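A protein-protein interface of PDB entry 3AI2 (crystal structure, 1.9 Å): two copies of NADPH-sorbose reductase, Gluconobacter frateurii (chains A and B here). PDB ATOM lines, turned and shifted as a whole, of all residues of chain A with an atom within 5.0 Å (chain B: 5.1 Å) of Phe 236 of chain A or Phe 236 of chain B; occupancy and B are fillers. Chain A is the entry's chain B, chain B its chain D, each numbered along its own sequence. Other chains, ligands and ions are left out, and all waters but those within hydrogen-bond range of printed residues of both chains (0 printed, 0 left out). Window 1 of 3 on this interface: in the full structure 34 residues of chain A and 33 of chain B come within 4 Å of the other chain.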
ATOM      1  N   ILE A 185       6.867 -10.534 -23.274  1.00  0.00           N
ATOM      2  CA  ILE A 185       7.941 -11.273 -22.567  1.00  0.00           C
ATOM      3  C   ILE A 185       9.133 -11.350 -23.517  1.00  0.00           C
ATOM      4  O   ILE A 185       8.939 -11.645 -24.670  1.00  0.00           O
ATOM      5  CB  ILE A 185       7.499 -12.735 -22.113  1.00  0.00           C
ATOM      6  CG1 ILE A 185       6.498 -12.657 -20.970  1.00  0.00           C
ATOM      7  CG2 ILE A 185       8.712 -13.589 -21.700  1.00  0.00           C
ATOM      8  CD1 ILE A 185       5.973 -14.053 -20.427  1.00  0.00           C
ATOM      9  N   GLU A 232      10.776 -23.836 -18.033  1.00  0.00           N
ATOM     10  CA  GLU A 232      11.209 -22.754 -17.159  1.00  0.00           C
ATOM     11  C   GLU A 232      10.549 -21.441 -17.592  1.00  0.00           C
ATOM     12  O   GLU A 232       9.910 -20.740 -16.789  1.00  0.00           O
ATOM     13  CB  GLU A 232      12.701 -22.588 -17.335  1.00  0.00           C
ATOM     14  CG  GLU A 232      13.393 -22.479 -16.096  1.00  0.00           C
ATOM     15  CD  GLU A 232      14.916 -22.514 -16.211  1.00  0.00           C
ATOM     16  OE1 GLU A 232      15.529 -23.005 -17.202  1.00  0.00           O
ATOM     17  OE2 GLU A 232      15.502 -22.033 -15.236  1.00  0.00           O
ATOM     18  N   LEU A 233      10.766 -21.091 -18.862  1.00  0.00           N
ATOM     19  CA  LEU A 233      10.136 -19.910 -19.489  1.00  0.00           C
ATOM     20  C   LEU A 233       8.611 -19.925 -19.368  1.00  0.00           C
ATOM     21  O   LEU A 233       7.955 -18.874 -19.077  1.00  0.00           O
ATOM     22  CB  LEU A 233      10.492 -19.872 -20.999  1.00  0.00           C
ATOM     23  CG  LEU A 233      10.057 -18.574 -21.716  1.00  0.00           C
ATOM     24  CD1 LEU A 233      10.515 -17.207 -21.017  1.00  0.00           C
ATOM     25  CD2 LEU A 233      10.527 -18.644 -23.155  1.00  0.00           C
ATOM     26  N   ALA A 234       8.013 -21.080 -19.687  1.00  0.00           N
ATOM     27  CA  ALA A 234       6.559 -21.145 -19.715  1.00  0.00           C
ATOM     28  C   ALA A 234       5.943 -20.709 -18.393  1.00  0.00           C
ATOM     29  O   ALA A 234       4.824 -20.160 -18.377  1.00  0.00           O
ATOM     30  CB  ALA A 234       6.075 -22.553 -20.070  1.00  0.00           C
ATOM     31  N   ASN A 235       6.598 -21.012 -17.285  1.00  0.00           N
ATOM     32  CA  ASN A 235       6.033 -20.565 -15.956  1.00  0.00           C
ATOM     33  C   ASN A 235       5.667 -19.077 -15.919  1.00  0.00           C
ATOM     34  O   ASN A 235       4.657 -18.722 -15.362  1.00  0.00           O
ATOM     35  CB  ASN A 235       7.013 -20.836 -14.839  1.00  0.00           C
ATOM     36  CG  ASN A 235       7.253 -22.338 -14.619  1.00  0.00           C
ATOM     37  OD1 ASN A 235       6.340 -23.153 -14.736  1.00  0.00           O
ATOM     38  ND2 ASN A 235       8.472 -22.682 -14.258  1.00  0.00           N
ATOM     39  N   PHE A 236       6.494 -18.235 -16.545  1.00  0.00           N
ATOM     40  CA  PHE A 236       6.308 -16.753 -16.518  1.00  0.00           C
ATOM     41  C   PHE A 236       5.146 -16.371 -17.389  1.00  0.00           C
ATOM     42  O   PHE A 236       4.358 -15.449 -17.032  1.00  0.00           O
ATOM     43  CB  PHE A 236       7.572 -16.036 -17.038  1.00  0.00           C
ATOM     44  CG  PHE A 236       7.876 -14.768 -16.328  1.00  0.00           C
ATOM     45  CD1 PHE A 236       8.964 -14.715 -15.444  1.00  0.00           C
ATOM     46  CD2 PHE A 236       7.075 -13.626 -16.516  1.00  0.00           C
ATOM     47  CE1 PHE A 236       9.268 -13.560 -14.726  1.00  0.00           C
ATOM     48  CE2 PHE A 236       7.364 -12.443 -15.817  1.00  0.00           C
ATOM     49  CZ  PHE A 236       8.459 -12.409 -14.920  1.00  0.00           C
ATOM     50  N   PHE A 237       5.007 -17.061 -18.526  1.00  0.00           N
ATOM     51  CA  PHE A 237       3.782 -16.911 -19.342  1.00  0.00           C
ATOM     52  C   PHE A 237       2.503 -17.221 -18.560  1.00  0.00           C
ATOM     53  O   PHE A 237       1.539 -16.402 -18.511  1.00  0.00           O
ATOM     54  CB  PHE A 237       3.806 -17.780 -20.629  1.00  0.00           C
ATOM     55  CG  PHE A 237       4.706 -17.217 -21.725  1.00  0.00           C
ATOM     56  CD1 PHE A 237       4.185 -16.418 -22.729  1.00  0.00           C
ATOM     57  CD2 PHE A 237       6.075 -17.470 -21.701  1.00  0.00           C
ATOM     58  CE1 PHE A 237       5.031 -15.882 -23.740  1.00  0.00           C
ATOM     59  CE2 PHE A 237       6.929 -16.939 -22.682  1.00  0.00           C
ATOM     60  CZ  PHE A 237       6.411 -16.150 -23.696  1.00  0.00           C
ATOM     61  N   VAL A 238       2.466 -18.380 -17.934  1.00  0.00           N
ATOM     62  CA  VAL A 238       1.250 -18.729 -17.187  1.00  0.00           C
ATOM     63  C   VAL A 238       1.009 -17.754 -16.025  1.00  0.00           C
ATOM     64  O   VAL A 238      -0.094 -17.263 -15.832  1.00  0.00           O
ATOM     65  CB  VAL A 238       1.370 -20.163 -16.631  1.00  0.00           C
ATOM     66  CG1 VAL A 238       0.164 -20.517 -15.762  1.00  0.00           C
ATOM     67  CG2 VAL A 238       1.554 -21.190 -17.752  1.00  0.00           C
ATOM     68  N   PHE A 239       2.046 -17.429 -15.270  1.00  0.00           N
ATOM     69  CA  PHE A 239       1.907 -16.422 -14.231  1.00  0.00           C
ATOM     70  C   PHE A 239       1.335 -15.098 -14.759  1.00  0.00           C
ATOM     71  O   PHE A 239       0.391 -14.524 -14.169  1.00  0.00           O
ATOM     72  CB  PHE A 239       3.230 -16.202 -13.508  1.00  0.00           C
ATOM     73  CG  PHE A 239       3.143 -15.161 -12.415  1.00  0.00           C
ATOM     74  CD1 PHE A 239       2.483 -15.453 -11.220  1.00  0.00           C
ATOM     75  CD2 PHE A 239       3.611 -13.867 -12.634  1.00  0.00           C
ATOM     76  CE1 PHE A 239       2.341 -14.492 -10.209  1.00  0.00           C
ATOM     77  CE2 PHE A 239       3.496 -12.902 -11.629  1.00  0.00           C
ATOM     78  CZ  PHE A 239       2.845 -13.212 -10.422  1.00  0.00           C
ATOM     79  N   LEU A 240       1.898 -14.569 -15.840  1.00  0.00           N
ATOM     80  CA  LEU A 240       1.456 -13.254 -16.303  1.00  0.00           C
ATOM     81  C   LEU A 240       0.019 -13.253 -16.813  1.00  0.00           C
ATOM     82  O   LEU A 240      -0.648 -12.211 -16.805  1.00  0.00           O
ATOM     83  CB  LEU A 240       2.410 -12.658 -17.347  1.00  0.00           C
ATOM     84  CG  LEU A 240       3.731 -12.106 -16.793  1.00  0.00           C
ATOM     85  CD1 LEU A 240       4.543 -11.589 -18.006  1.00  0.00           C
ATOM     86  CD2 LEU A 240       3.502 -10.943 -15.711  1.00  0.00           C
ATOM     87  N   CYS A 241      -0.455 -14.389 -17.297  1.00  0.00           N
ATOM     88  CA  CYS A 241      -1.837 -14.490 -17.766  1.00  0.00           C
ATOM     89  C   CYS A 241      -2.788 -14.945 -16.638  1.00  0.00           C
ATOM     90  O   CYS A 241      -3.927 -15.273 -16.921  1.00  0.00           O
ATOM     91  CB  CYS A 241      -1.910 -15.521 -18.914  1.00  0.00           C
ATOM     92  SG  CYS A 241      -1.018 -14.945 -20.384  1.00  0.00           S
ATOM     93  N   SER A 248      -0.241  -6.037 -13.880  1.00  0.00           N
ATOM     94  CA  SER A 248       0.725  -5.971 -14.978  1.00  0.00           C
ATOM     95  C   SER A 248       0.048  -5.503 -16.254  1.00  0.00           C
ATOM     96  O   SER A 248      -0.818  -6.181 -16.769  1.00  0.00           O
ATOM     97  CB  SER A 248       1.421  -7.331 -15.164  1.00  0.00           C
ATOM     98  OG  SER A 248       2.136  -7.647 -13.999  1.00  0.00           O
ATOM     99  N   TYR A 253       8.776  -7.957 -19.811  1.00  0.00           N
ATOM    100  CA  TYR A 253       9.398  -8.724 -18.738  1.00  0.00           C
ATOM    101  C   TYR A 253      10.499  -9.624 -19.348  1.00  0.00           C
ATOM    102  O   TYR A 253      10.216 -10.517 -20.202  1.00  0.00           O
ATOM    103  CB  TYR A 253       8.323  -9.612 -18.074  1.00  0.00           C
ATOM    104  CG  TYR A 253       7.252  -8.798 -17.343  1.00  0.00           C
ATOM    105  CD1 TYR A 253       7.530  -8.244 -16.106  1.00  0.00           C
ATOM    106  CD2 TYR A 253       5.978  -8.585 -17.883  1.00  0.00           C
ATOM    107  CE1 TYR A 253       6.612  -7.502 -15.422  1.00  0.00           C
ATOM    108  CE2 TYR A 253       4.987  -7.839 -17.158  1.00  0.00           C
ATOM    109  CZ  TYR A 253       5.338  -7.322 -15.910  1.00  0.00           C
ATOM    110  OH  TYR A 253       4.492  -6.564 -15.129  1.00  0.00           O
ATOM    111  N   VAL A 255      13.279 -12.574 -19.431  1.00  0.00           N
ATOM    112  CA  VAL A 255      13.529 -13.834 -18.735  1.00  0.00           C
ATOM    113  C   VAL A 255      14.771 -14.387 -19.401  1.00  0.00           C
ATOM    114  O   VAL A 255      14.654 -15.076 -20.429  1.00  0.00           O
ATOM    115  CB  VAL A 255      12.345 -14.827 -18.865  1.00  0.00           C
ATOM    116  CG1 VAL A 255      12.608 -16.090 -18.029  1.00  0.00           C
ATOM    117  CG2 VAL A 255      11.004 -14.172 -18.411  1.00  0.00           C
ATOM    118  N   ILE B 185      12.156  -5.270  -8.435  1.00  0.00           N
ATOM    119  CA  ILE B 185      10.768  -5.021  -8.803  1.00  0.00           C
ATOM    120  C   ILE B 185      10.523  -3.522  -8.668  1.00  0.00           C
ATOM    121  O   ILE B 185      10.887  -2.941  -7.644  1.00  0.00           O
ATOM    122  CB  ILE B 185       9.719  -5.844  -7.942  1.00  0.00           C
ATOM    123  CG1 ILE B 185       9.768  -7.329  -8.319  1.00  0.00           C
ATOM    124  CG2 ILE B 185       8.254  -5.346  -8.180  1.00  0.00           C
ATOM    125  CD1 ILE B 185       8.907  -8.280  -7.430  1.00  0.00           C
ATOM    126  N   GLU B 232      -1.854  -7.690  -4.466  1.00  0.00           N
ATOM    127  CA  GLU B 232      -1.635  -7.901  -5.901  1.00  0.00           C
ATOM    128  C   GLU B 232      -0.157  -7.835  -6.197  1.00  0.00           C
ATOM    129  O   GLU B 232       0.408  -8.658  -6.908  1.00  0.00           O
ATOM    130  CB  GLU B 232      -2.261  -6.767  -6.697  1.00  0.00           C
ATOM    131  CG  GLU B 232      -3.510  -7.044  -7.298  1.00  0.00           C
ATOM    132  CD  GLU B 232      -3.997  -5.840  -8.100  1.00  0.00           C
ATOM    133  OE1 GLU B 232      -4.274  -5.992  -9.318  1.00  0.00           O
ATOM    134  OE2 GLU B 232      -4.111  -4.760  -7.499  1.00  0.00           O
ATOM    135  N   LEU B 233       0.478  -6.799  -5.692  1.00  0.00           N
ATOM    136  CA  LEU B 233       1.917  -6.682  -5.862  1.00  0.00           C
ATOM    137  C   LEU B 233       2.693  -7.833  -5.208  1.00  0.00           C
ATOM    138  O   LEU B 233       3.679  -8.310  -5.753  1.00  0.00           O
ATOM    139  CB  LEU B 233       2.388  -5.360  -5.230  1.00  0.00           C
ATOM    140  CG  LEU B 233       3.878  -5.122  -5.390  1.00  0.00           C
ATOM    141  CD1 LEU B 233       4.334  -5.087  -6.882  1.00  0.00           C
ATOM    142  CD2 LEU B 233       4.221  -3.817  -4.683  1.00  0.00           C
ATOM    143  N   ALA B 234       2.307  -8.207  -3.997  1.00  0.00           N
ATOM    144  CA  ALA B 234       3.003  -9.292  -3.285  1.00  0.00           C
ATOM    145  C   ALA B 234       3.111 -10.535  -4.144  1.00  0.00           C
ATOM    146  O   ALA B 234       4.129 -11.228  -4.088  1.00  0.00           O
ATOM    147  CB  ALA B 234       2.260  -9.642  -1.926  1.00  0.00           C
ATOM    148  N   ASN B 235       2.090 -10.840  -4.920  1.00  0.00           N
ATOM    149  CA  ASN B 235       2.149 -12.087  -5.740  1.00  0.00           C
ATOM    150  C   ASN B 235       3.384 -12.147  -6.585  1.00  0.00           C
ATOM    151  O   ASN B 235       3.972 -13.222  -6.789  1.00  0.00           O
ATOM    152  CB  ASN B 235       0.922 -12.213  -6.659  1.00  0.00           C
ATOM    153  CG  ASN B 235      -0.374 -12.280  -5.887  1.00  0.00           C
ATOM    154  OD1 ASN B 235      -0.463 -12.934  -4.842  1.00  0.00           O
ATOM    155  ND2 ASN B 235      -1.388 -11.649  -6.405  1.00  0.00           N
ATOM    156  N   PHE B 236       3.781 -10.993  -7.100  1.00  0.00           N
ATOM    157  CA  PHE B 236       4.903 -10.953  -8.000  1.00  0.00           C
ATOM    158  C   PHE B 236       6.223 -11.210  -7.256  1.00  0.00           C
ATOM    159  O   PHE B 236       7.106 -11.904  -7.791  1.00  0.00           O
ATOM    160  CB  PHE B 236       4.980  -9.586  -8.726  1.00  0.00           C
ATOM    161  CG  PHE B 236       5.532  -9.685 -10.108  1.00  0.00           C
ATOM    162  CD1 PHE B 236       4.686  -9.561 -11.197  1.00  0.00           C
ATOM    163  CD2 PHE B 236       6.902  -9.908 -10.325  1.00  0.00           C
ATOM    164  CE1 PHE B 236       5.184  -9.687 -12.510  1.00  0.00           C
ATOM    165  CE2 PHE B 236       7.423 -10.011 -11.645  1.00  0.00           C
ATOM    166  CZ  PHE B 236       6.551  -9.909 -12.723  1.00  0.00           C
ATOM    167  N   PHE B 237       6.332 -10.700  -6.029  1.00  0.00           N
ATOM    168  CA  PHE B 237       7.509 -10.926  -5.205  1.00  0.00           C
ATOM    169  C   PHE B 237       7.609 -12.399  -4.867  1.00  0.00           C
ATOM    170  O   PHE B 237       8.687 -12.985  -4.935  1.00  0.00           O
ATOM    171  CB  PHE B 237       7.495 -10.141  -3.868  1.00  0.00           C
ATOM    172  CG  PHE B 237       7.851  -8.702  -3.981  1.00  0.00           C
ATOM    173  CD1 PHE B 237       9.139  -8.255  -3.670  1.00  0.00           C
ATOM    174  CD2 PHE B 237       6.898  -7.779  -4.430  1.00  0.00           C
ATOM    175  CE1 PHE B 237       9.471  -6.883  -3.773  1.00  0.00           C
ATOM    176  CE2 PHE B 237       7.226  -6.419  -4.584  1.00  0.00           C
ATOM    177  CZ  PHE B 237       8.494  -5.957  -4.230  1.00  0.00           C
ATOM    178  N   VAL B 238       6.474 -13.014  -4.543  1.00  0.00           N
ATOM    179  CA  VAL B 238       6.472 -14.449  -4.185  1.00  0.00           C
ATOM    180  C   VAL B 238       6.871 -15.269  -5.429  1.00  0.00           C
ATOM    181  O   VAL B 238       7.732 -16.163  -5.338  1.00  0.00           O
ATOM    182  CB  VAL B 238       5.094 -14.815  -3.664  1.00  0.00           C
ATOM    183  CG1 VAL B 238       4.918 -16.299  -3.476  1.00  0.00           C
ATOM    184  CG2 VAL B 238       4.857 -14.054  -2.271  1.00  0.00           C
ATOM    185  N   PHE B 239       6.282 -14.936  -6.579  1.00  0.00           N
ATOM    186  CA  PHE B 239       6.611 -15.690  -7.796  1.00  0.00           C
ATOM    187  C   PHE B 239       8.088 -15.591  -8.146  1.00  0.00           C
ATOM    188  O   PHE B 239       8.774 -16.606  -8.456  1.00  0.00           O
ATOM    189  CB  PHE B 239       5.743 -15.247  -8.981  1.00  0.00           C
ATOM    190  CG  PHE B 239       6.109 -15.945 -10.272  1.00  0.00           C
ATOM    191  CD1 PHE B 239       5.732 -17.275 -10.511  1.00  0.00           C
ATOM    192  CD2 PHE B 239       6.849 -15.283 -11.237  1.00  0.00           C
ATOM    193  CE1 PHE B 239       6.076 -17.926 -11.691  1.00  0.00           C
ATOM    194  CE2 PHE B 239       7.216 -15.931 -12.437  1.00  0.00           C
ATOM    195  CZ  PHE B 239       6.835 -17.240 -12.667  1.00  0.00           C
ATOM    196  N   LEU B 240       8.612 -14.363  -8.101  1.00  0.00           N
ATOM    197  CA  LEU B 240      10.003 -14.197  -8.487  1.00  0.00           C
ATOM    198  C   LEU B 240      10.957 -14.877  -7.536  1.00  0.00           C
ATOM    199  O   LEU B 240      12.095 -15.144  -7.917  1.00  0.00           O
ATOM    200  CB  LEU B 240      10.391 -12.742  -8.583  1.00  0.00           C
ATOM    201  CG  LEU B 240      10.202 -11.961  -9.870  1.00  0.00           C
ATOM    202  CD1 LEU B 240      11.000 -10.660  -9.625  1.00  0.00           C
ATOM    203  CD2 LEU B 240      10.702 -12.718 -11.097  1.00  0.00           C
ATOM    204  N   CYS B 241      10.538 -15.124  -6.292  1.00  0.00           N
ATOM    205  CA  CYS B 241      11.427 -15.797  -5.349  1.00  0.00           C
ATOM    206  C   CYS B 241      11.187 -17.304  -5.346  1.00  0.00           C
ATOM    207  O   CYS B 241      11.739 -17.999  -4.496  1.00  0.00           O
ATOM    208  CB  CYS B 241      11.316 -15.207  -3.911  1.00  0.00           C
ATOM    209  SG  CYS B 241      11.861 -13.472  -3.815  1.00  0.00           S
ATOM    210  N   SER B 248      15.170 -16.014 -14.064  1.00  0.00           N
ATOM    211  CA  SER B 248      15.150 -14.548 -13.873  1.00  0.00           C
ATOM    212  C   SER B 248      16.397 -14.127 -13.083  1.00  0.00           C
ATOM    213  O   SER B 248      16.514 -14.503 -11.938  1.00  0.00           O
ATOM    214  CB  SER B 248      13.866 -14.164 -13.114  1.00  0.00           C
ATOM    215  OG  SER B 248      12.747 -14.416 -13.938  1.00  0.00           O
ATOM    216  N   TYR B 253      11.567  -5.746 -13.047  1.00  0.00           N
ATOM    217  CA  TYR B 253      10.198  -6.095 -13.401  1.00  0.00           C
ATOM    218  C   TYR B 253       9.246  -5.023 -12.921  1.00  0.00           C
ATOM    219  O   TYR B 253       9.128  -4.787 -11.683  1.00  0.00           O
ATOM    220  CB  TYR B 253       9.815  -7.433 -12.744  1.00  0.00           C
ATOM    221  CG  TYR B 253      10.598  -8.596 -13.330  1.00  0.00           C
ATOM    222  CD1 TYR B 253      10.417  -8.995 -14.655  1.00  0.00           C
ATOM    223  CD2 TYR B 253      11.548  -9.274 -12.576  1.00  0.00           C
ATOM    224  CE1 TYR B 253      11.139 -10.082 -15.204  1.00  0.00           C
ATOM    225  CE2 TYR B 253      12.277 -10.329 -13.133  1.00  0.00           C
ATOM    226  CZ  TYR B 253      12.030 -10.745 -14.419  1.00  0.00           C
ATOM    227  OH  TYR B 253      12.783 -11.760 -14.922  1.00  0.00           O
ATOM    228  N   PHE B 254       8.535  -4.393 -13.863  1.00  0.00           N
ATOM    229  CA  PHE B 254       7.589  -3.327 -13.484  1.00  0.00           C
ATOM    230  C   PHE B 254       6.216  -3.909 -13.169  1.00  0.00           C
ATOM    231  O   PHE B 254       5.744  -4.837 -13.833  1.00  0.00           O
ATOM    232  CB  PHE B 254       7.486  -2.245 -14.579  1.00  0.00           C
ATOM    233  CG  PHE B 254       8.722  -1.399 -14.708  1.00  0.00           C
ATOM    234  CD1 PHE B 254       8.770  -0.119 -14.163  1.00  0.00           C
ATOM    235  CD2 PHE B 254       9.852  -1.907 -15.309  1.00  0.00           C
ATOM    236  CE1 PHE B 254       9.881   0.658 -14.254  1.00  0.00           C
ATOM    237  CE2 PHE B 254      11.006  -1.140 -15.377  1.00  0.00           C
ATOM    238  CZ  PHE B 254      11.015   0.143 -14.851  1.00  0.00           C
ATOM    239  N   VAL B 255       5.596  -3.421 -12.106  1.00  0.00           N
ATOM    240  CA  VAL B 255       4.256  -3.859 -11.781  1.00  0.00           C
ATOM    241  C   VAL B 255       3.470  -2.559 -11.525  1.00  0.00           C
ATOM    242  O   VAL B 255       3.447  -2.067 -10.394  1.00  0.00           O
ATOM    243  CB  VAL B 255       4.220  -4.832 -10.561  1.00  0.00           C
ATOM    244  CG1 VAL B 255       2.764  -5.300 -10.308  1.00  0.00           C
ATOM    245  CG2 VAL B 255       5.160  -6.017 -10.785  1.00  0.00           C
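The side-chain hydroxyl (OH) of Tyr 253 of chain A sits at hydrogen-bond distance from the backbone carbonyl oxygen (O) of Phe 254 of chain B, at 2.5 Å.
O of Glu 232 of chain A lies close to ND2 of Asn 235 of chain A (3.5 Å). The side-chain hydroxyl (OG) of Ser 248 of chain B lies within hydrogen-bond range of the side-chain hydroxyl (OH) of Tyr 253 of chain B (2.8 Å). The side-chain hydroxyl (OG) of Ser 248 of chain A lies within hydrogen-bond range of the side-chain hydroxyl (OH) of Tyr 253 of chain A (2.8 Å).
Phe 236 of chain A touches Phe 236 of chain B. Phe 236 of chain A touches Phe 239 of chain B. Phe 236 of chain A touches Leu 240 of chain B. Ser 248 of chain B touches Phe 236 of chain A. Tyr 253 of chain B touches Phe 236 of chain A. Phe 239 of chain A touches Asn 235 of chain B (CZ to O, 3.8 Å). Phe 239 of chain A touches Phe 239 of chain B. Leu 240 of chain A touches Phe 236 of chain B. Phe 236 of chain B touches Ser 248 of chain A. CD1 of Tyr 253 of chain A touches CD1 of Tyr 253 of chain B (3.3 Å).
Of the printed residues of chain B, Phe 236 of chain A touches Phe 236 (3.8 Å), Phe 239 (3.7 Å), Leu 240 (3.99 Å), Ser 248 (3.7 Å) and Tyr 253 (3.6 Å). Of the printed residues of chain B, Leu 240 of chain A touches Phe 236 (3.8 Å). Printed residues of chain B within 4 Å of Ser 248 of chain A: Phe 236. Of the printed residues of chain A, Asn 235 of chain B touches Phe 239 (3.8 Å). Of the printed residues of chain A, Phe 236 of chain B touches Phe 236, Phe 239, Leu 240, Ser 248 and Tyr 253. Printed residues of chain A within 4 Å of Phe 239 of chain B: Asn 235, Phe 236 and Phe 239. Printed residues of chain A within 4 Å of Phe 254 of chain B: Tyr 253. The nearest printed residue of chain B that does not touch Phe 236 of chain A is Phe 254 of chain B (8.0 Å). The nearest printed residue of chain A that does not touch Phe 236 of chain B is Val 255 of chain A (8.4 Å).
Of the 14 printed residues of chain A, 6 touch a printed residue of chain B.
Asn 235 of chain A touches Phe 239 of chain B, and with the chains exchanged Phe 239 of chain A touches Asn 235 of chain B. Phe 236 of chain A touches its own counterpart, Phe 236 of chain B. Phe 236 of chain A touches Leu 240 of chain B, and with the chains exchanged Leu 240 of chain A touches Phe 236 of chain B. Phe 236 of chain A touches Ser 248 of chain B, and with the chains exchanged Ser 248 of chain A touches Phe 236 of chain B. 14 positions are printed for both chains.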
